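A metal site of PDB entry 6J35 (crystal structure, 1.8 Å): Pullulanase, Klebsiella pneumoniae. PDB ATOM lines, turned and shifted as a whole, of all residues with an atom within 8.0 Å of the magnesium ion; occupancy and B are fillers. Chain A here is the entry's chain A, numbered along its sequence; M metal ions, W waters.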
ATOM      1  N   SER A 929       0.679 -21.661 -18.887  1.00  0.00           N
ATOM      2  CA  SER A 929      -0.053 -21.588 -17.607  1.00  0.00           C
ATOM      3  C   SER A 929      -0.922 -20.342 -17.559  1.00  0.00           C
ATOM      4  O   SER A 929      -0.475 -19.252 -17.946  1.00  0.00           O
ATOM      5  CB  SER A 929       0.896 -21.574 -16.405  1.00  0.00           C
ATOM      6  OG  SER A 929       0.178 -21.429 -15.183  1.00  0.00           O
ATOM      7  N   PRO A 930      -2.154 -20.456 -17.074  1.00  0.00           N
ATOM      8  CA  PRO A 930      -2.982 -19.265 -16.851  1.00  0.00           C
ATOM      9  C   PRO A 930      -2.464 -18.316 -15.776  1.00  0.00           C
ATOM     10  O   PRO A 930      -2.987 -17.193 -15.664  1.00  0.00           O
ATOM     11  CB  PRO A 930      -4.342 -19.862 -16.440  1.00  0.00           C
ATOM     12  CG  PRO A 930      -4.017 -21.178 -15.845  1.00  0.00           C
ATOM     13  CD  PRO A 930      -2.870 -21.700 -16.711  1.00  0.00           C
ATOM     14  N   LEU A 931      -1.493 -18.727 -14.953  1.00  0.00           N
ATOM     15  CA  LEU A 931      -0.987 -17.804 -13.939  1.00  0.00           C
ATOM     16  C   LEU A 931      -0.230 -16.629 -14.571  1.00  0.00           C
ATOM     17  O   LEU A 931      -0.134 -15.560 -13.958  1.00  0.00           O
ATOM     18  CB  LEU A 931      -0.110 -18.564 -12.930  1.00  0.00           C
ATOM     19  CG  LEU A 931      -0.827 -19.696 -12.189  1.00  0.00           C
ATOM     20  CD1 LEU A 931       0.162 -20.605 -11.467  1.00  0.00           C
ATOM     21  CD2 LEU A 931      -1.848 -19.135 -11.204  1.00  0.00           C
ATOM     22  N   ARG A 943      -2.313 -12.315  -6.100  1.00  0.00           N
ATOM     23  CA  ARG A 943      -1.434 -13.441  -6.415  1.00  0.00           C
ATOM     24  C   ARG A 943       0.004 -13.058  -6.745  1.00  0.00           C
ATOM     25  O   ARG A 943       0.888 -13.901  -6.573  1.00  0.00           O
ATOM     26  CB  ARG A 943      -2.006 -14.258  -7.586  1.00  0.00           C
ATOM     27  CG  ARG A 943      -3.347 -14.932  -7.303  1.00  0.00           C
ATOM     28  CD  ARG A 943      -3.877 -15.667  -8.544  1.00  0.00           C
ATOM     29  NE  ARG A 943      -5.150 -16.330  -8.261  1.00  0.00           N
ATOM     30  CZ  ARG A 943      -5.329 -17.639  -8.127  1.00  0.00           C
ATOM     31  NH1 ARG A 943      -4.323 -18.476  -8.285  1.00  0.00           N
ATOM     32  NH2 ARG A 943      -6.544 -18.135  -7.887  1.00  0.00           N
ATOM     33  N   ASP A 963       1.068 -16.658  -7.116  1.00  0.00           N
ATOM     34  CA  ASP A 963       0.493 -17.641  -6.208  1.00  0.00           C
ATOM     35  C   ASP A 963      -0.625 -18.431  -6.884  1.00  0.00           C
ATOM     36  O   ASP A 963      -1.503 -17.845  -7.528  1.00  0.00           O
ATOM     37  CB  ASP A 963      -0.043 -16.901  -4.980  1.00  0.00           C
ATOM     38  CG  ASP A 963      -0.372 -17.818  -3.823  1.00  0.00           C
ATOM     39  OD1 ASP A 963      -0.012 -19.019  -3.855  1.00  0.00           O
ATOM     40  OD2 ASP A 963      -0.998 -17.294  -2.871  1.00  0.00           O
ATOM     41  N   ASP A 964      -0.593 -19.759  -6.744  1.00  0.00           N
ATOM     42  CA  ASP A 964      -1.773 -20.569  -7.022  1.00  0.00           C
ATOM     43  C   ASP A 964      -2.230 -21.361  -5.790  1.00  0.00           C
ATOM     44  O   ASP A 964      -3.036 -22.292  -5.936  1.00  0.00           O
ATOM     45  CB  ASP A 964      -1.544 -21.525  -8.201  1.00  0.00           C
ATOM     46  CG  ASP A 964      -2.842 -21.874  -8.938  1.00  0.00           C
ATOM     47  OD1 ASP A 964      -3.748 -21.010  -9.007  1.00  0.00           O
ATOM     48  OD2 ASP A 964      -2.976 -23.026  -9.435  1.00  0.00           O
ATOM     49  N   GLY A 965      -1.720 -21.016  -4.597  1.00  0.00           N
ATOM     50  CA  GLY A 965      -2.042 -21.759  -3.391  1.00  0.00           C
ATOM     51  C   GLY A 965      -3.299 -21.280  -2.677  1.00  0.00           C
ATOM     52  O   GLY A 965      -4.000 -20.356  -3.095  1.00  0.00           O
ATOM     53  N   ALA A 970      -8.902 -20.212  -5.706  1.00  0.00           N
ATOM     54  CA  ALA A 970      -8.928 -21.515  -6.334  1.00  0.00           C
ATOM     55  C   ALA A 970      -7.652 -21.763  -7.120  1.00  0.00           C
ATOM     56  O   ALA A 970      -6.960 -20.834  -7.539  1.00  0.00           O
ATOM     57  CB  ALA A 970     -10.147 -21.636  -7.261  1.00  0.00           C
ATOM     58  N   SER A 971      -7.343 -23.032  -7.322  1.00  0.00           N
ATOM     59  CA  SER A 971      -6.241 -23.399  -8.210  1.00  0.00           C
ATOM     60  C   SER A 971      -6.668 -23.151  -9.652  1.00  0.00           C
ATOM     61  O   SER A 971      -7.654 -23.717 -10.121  1.00  0.00           O
ATOM     62  CB  SER A 971      -5.871 -24.872  -7.998  1.00  0.00           C
ATOM     63  OG  SER A 971      -4.960 -25.347  -8.978  1.00  0.00           O
ATOM     64  N   LEU A 972      -5.933 -22.272 -10.338  1.00  0.00           N
ATOM     65  CA  LEU A 972      -6.169 -21.995 -11.748  1.00  0.00           C
ATOM     66  C   LEU A 972      -5.397 -22.932 -12.659  1.00  0.00           C
ATOM     67  O   LEU A 972      -5.700 -22.984 -13.857  1.00  0.00           O
ATOM     68  CB  LEU A 972      -5.778 -20.553 -12.057  1.00  0.00           C
ATOM     69  CG  LEU A 972      -6.457 -19.477 -11.228  1.00  0.00           C
ATOM     70  CD1 LEU A 972      -5.886 -18.129 -11.644  1.00  0.00           C
ATOM     71  CD2 LEU A 972      -7.963 -19.532 -11.486  1.00  0.00           C
ATOM     72  N   ASP A 973      -4.450 -23.681 -12.114  1.00  0.00           N
ATOM     73  CA  ASP A 973      -3.528 -24.504 -12.884  1.00  0.00           C
ATOM     74  C   ASP A 973      -3.332 -25.778 -12.073  1.00  0.00           C
ATOM     75  O   ASP A 973      -2.726 -25.732 -10.989  1.00  0.00           O
ATOM     76  CB  ASP A 973      -2.208 -23.747 -13.106  1.00  0.00           C
ATOM     77  CG  ASP A 973      -1.202 -24.498 -13.974  1.00  0.00           C
ATOM     78  OD1 ASP A 973      -1.350 -25.717 -14.211  1.00  0.00           O
ATOM     79  OD2 ASP A 973      -0.237 -23.829 -14.413  1.00  0.00           O
ATOM     80  N   SER A 974      -3.859 -26.900 -12.554  1.00  0.00           N
ATOM     81  CA  SER A 974      -3.804 -28.128 -11.768  1.00  0.00           C
ATOM     82  C   SER A 974      -2.399 -28.687 -11.615  1.00  0.00           C
ATOM     83  O   SER A 974      -2.173 -29.552 -10.756  1.00  0.00           O
ATOM     84  CB  SER A 974      -4.723 -29.191 -12.412  1.00  0.00           C
ATOM     85  OG  SER A 974      -4.230 -29.564 -13.683  1.00  0.00           O
ATOM     86  N   ARG A 975      -1.441 -28.235 -12.425  1.00  0.00           N
ATOM     87  CA  ARG A 975      -0.097 -28.792 -12.379  1.00  0.00           C
ATOM     88  C   ARG A 975       0.796 -28.143 -11.347  1.00  0.00           C
ATOM     89  O   ARG A 975       1.759 -28.775 -10.918  1.00  0.00           O
ATOM     90  CB  ARG A 975       0.570 -28.679 -13.757  1.00  0.00           C
ATOM     91  CG  ARG A 975      -0.182 -29.428 -14.841  1.00  0.00           C
ATOM     92  CD  ARG A 975       0.661 -29.694 -16.064  1.00  0.00           C
ATOM     93  NE  ARG A 975      -0.123 -30.320 -17.128  1.00  0.00           N
ATOM     94  CZ  ARG A 975       0.377 -30.683 -18.305  1.00  0.00           C
ATOM     95  NH1 ARG A 975      -0.401 -31.261 -19.215  1.00  0.00           N
ATOM     96  NH2 ARG A 975       1.681 -30.474 -18.564  1.00  0.00           N
ATOM     97  N   VAL A 976       0.521 -26.907 -10.924  1.00  0.00           N
ATOM     98  CA  VAL A 976       1.436 -26.173 -10.057  1.00  0.00           C
ATOM     99  C   VAL A 976       0.647 -25.424  -8.991  1.00  0.00           C
ATOM    100  O   VAL A 976      -0.524 -25.077  -9.174  1.00  0.00           O
ATOM    101  CB  VAL A 976       2.340 -25.167 -10.811  1.00  0.00           C
ATOM    102  CG1 VAL A 976       3.070 -25.832 -11.984  1.00  0.00           C
ATOM    103  CG2 VAL A 976       1.555 -23.951 -11.282  1.00  0.00           C
ATOM    104  N   ASP A 977       1.337 -25.147  -7.884  1.00  0.00           N
ATOM    105  CA  ASP A 977       0.838 -24.334  -6.774  1.00  0.00           C
ATOM    106  C   ASP A 977       1.402 -22.928  -6.799  1.00  0.00           C
ATOM    107  O   ASP A 977       1.063 -22.113  -5.934  1.00  0.00           O
ATOM    108  CB  ASP A 977       1.190 -24.993  -5.437  1.00  0.00           C
ATOM    109  CG  ASP A 977       0.278 -26.163  -5.097  1.00  0.00           C
ATOM    110  OD1 ASP A 977      -0.933 -26.113  -5.406  1.00  0.00           O
ATOM    111  OD2 ASP A 977       0.781 -27.142  -4.500  1.00  0.00           O
ATOM    112  N   GLY A 978       2.252 -22.623  -7.759  1.00  0.00           N
ATOM    113  CA  GLY A 978       2.859 -21.316  -7.827  1.00  0.00           C
ATOM    114  C   GLY A 978       3.986 -21.297  -8.839  1.00  0.00           C
ATOM    115  O   GLY A 978       4.490 -22.354  -9.229  1.00  0.00           O
ATOM    116  N   LEU A1038       6.130 -24.728  -8.226  1.00  0.00           N
ATOM    117  CA  LEU A1038       5.835 -25.626  -7.130  1.00  0.00           C
ATOM    118  C   LEU A1038       4.905 -26.704  -7.653  1.00  0.00           C
ATOM    119  O   LEU A1038       3.750 -26.397  -7.989  1.00  0.00           O
ATOM    120  CB  LEU A1038       5.175 -24.862  -5.979  1.00  0.00           C
ATOM    121  CG  LEU A1038       6.022 -23.791  -5.279  1.00  0.00           C
ATOM    122  CD1 LEU A1038       5.183 -23.046  -4.259  1.00  0.00           C
ATOM    123  CD2 LEU A1038       7.268 -24.412  -4.615  1.00  0.00           C
ATOM    124  N   PRO A1039       5.335 -27.958  -7.765  1.00  0.00           N
ATOM    125  CA  PRO A1039       4.448 -28.995  -8.313  1.00  0.00           C
ATOM    126  C   PRO A1039       3.232 -29.205  -7.414  1.00  0.00           C
ATOM    127  O   PRO A1039       3.350 -29.236  -6.195  1.00  0.00           O
ATOM    128  CB  PRO A1039       5.336 -30.252  -8.328  1.00  0.00           C
ATOM    129  CG  PRO A1039       6.329 -30.003  -7.235  1.00  0.00           C
ATOM    130  CD  PRO A1039       6.607 -28.522  -7.278  1.00  0.00           C
ATOM    131  N   GLN A1040       2.056 -29.357  -8.042  1.00  0.00           N
ATOM    132  CA  GLN A1040       0.828 -29.517  -7.265  1.00  0.00           C
ATOM    133  C   GLN A1040       0.568 -30.997  -7.006  1.00  0.00           C
ATOM    134  O   GLN A1040       0.695 -31.823  -7.921  1.00  0.00           O
ATOM    135  CB  GLN A1040      -0.368 -28.902  -7.982  1.00  0.00           C
ATOM    136  CG  GLN A1040      -1.652 -28.851  -7.145  1.00  0.00           C
ATOM    137  CD  GLN A1040      -2.738 -28.034  -7.815  1.00  0.00           C
ATOM    138  OE1 GLN A1040      -2.427 -27.109  -8.579  1.00  0.00           O
ATOM    139  NE2 GLN A1040      -3.999 -28.362  -7.557  1.00  0.00           N
ATOM    140  N   GLY A1041       0.237 -31.323  -5.764  1.00  0.00           N
ATOM    141  CA  GLY A1041       0.018 -32.698  -5.355  1.00  0.00           C
ATOM    142  C   GLY A1041      -1.452 -33.049  -5.282  1.00  0.00           C
ATOM    143  O   GLY A1041      -2.268 -32.572  -6.078  1.00  0.00           O
ATOM    144  N   SER A1043      -3.861 -32.299  -3.181  1.00  0.00           N
ATOM    145  CA  SER A1043      -4.701 -31.128  -3.041  1.00  0.00           C
ATOM    146  C   SER A1043      -3.893 -29.874  -3.321  1.00  0.00           C
ATOM    147  O   SER A1043      -2.658 -29.879  -3.274  1.00  0.00           O
ATOM    148  CB  SER A1043      -5.293 -31.025  -1.616  1.00  0.00           C
ATOM    149  OG  SER A1043      -5.818 -32.259  -1.182  1.00  0.00           O
ATOM    150  N   GLN A1044      -4.602 -28.778  -3.575  1.00  0.00           N
ATOM    151  CA  GLN A1044      -3.971 -27.479  -3.623  1.00  0.00           C
ATOM    152  C   GLN A1044      -3.102 -27.256  -2.384  1.00  0.00           C
ATOM    153  O   GLN A1044      -3.509 -27.578  -1.253  1.00  0.00           O
ATOM    154  CB  GLN A1044      -5.042 -26.394  -3.746  1.00  0.00           C
ATOM    155  CG  GLN A1044      -4.513 -24.973  -3.771  1.00  0.00           C
ATOM    156  CD  GLN A1044      -5.618 -23.938  -3.831  1.00  0.00           C
ATOM    157  OE1 GLN A1044      -6.640 -24.062  -3.159  1.00  0.00           O
ATOM    158  NE2 GLN A1044      -5.403 -22.901  -4.625  1.00  0.00           N
ATOM    159  N   GLY A1045      -1.902 -26.714  -2.591  1.00  0.00           N
ATOM    160  CA  GLY A1045      -0.933 -26.525  -1.538  1.00  0.00           C
ATOM    161  C   GLY A1045      -0.793 -25.086  -1.075  1.00  0.00           C
ATOM    162  O   GLY A1045      -1.609 -24.215  -1.372  1.00  0.00           O
HETATM  163 MG    MG M   1      -2.679 -25.063  -9.019  1.00  0.00          MG
HETATM  164  O   HOH W   1      -2.678 -24.785  -6.939  1.00  0.00           O
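Water W1 lies within hydrogen-bond range of the side-chain carboxylate (OD1) of Asp 977 and the backbone carbonyl oxygen (O) of Asp 964.
Within 4 Å of the magnesium ion: Asp 964, Ser 971, Asp 973, Val 976 and Gln 1040.
The nearest printed residue that does not touch the magnesium ion is Asp 977 (4.1 Å).
The side-chain amide oxygen (OE1) of Gln 1040 lies close to the backbone carbonyl oxygen (O) of Ser 974.
The side-chain carboxylate (OD1) of Asp 964 lies within hydrogen-bond range of the backbone NH (N) of Leu 972.
The backbone carbonyl oxygen (O) of Arg 975 sits at hydrogen-bond distance from the backbone NH (N) of Gln 1040.
The backbone NH (N) of Ser 971 lies close to the side-chain amide nitrogen (NE2) of Gln 1044.
NH1 of Arg 943 is in salt-bridge range of OD1 of Asp 964.
The backbone carbonyl oxygen (O) of Asp 964 is in hydrogen-bond range of the side-chain amide nitrogen (NE2) of Gln 1044 (2.8 Å).
OD1 of Asp 973 sits at hydrogen-bond distance from N of Arg 975, at 3.1 Å.
The backbone NH (N) of Asp 964 is in hydrogen-bond range of the backbone carbonyl oxygen (O) of Asp 977, 3.0 Å away.
The magnesium ion is bound by O of Asp 973 (2.1 Å).
The magnesium ion is bound by water W1 (2.1 Å).
The side-chain carboxylate (OD2) of Asp 964 binds the magnesium ion (2.1 Å).
The magnesium ion is bound by OE1 of Gln 1040 (2.1 Å).
O of Val 976 binds the magnesium ion (2.2 Å).
The magnesium ion is bound by OG of Ser 971 (2.3 Å).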
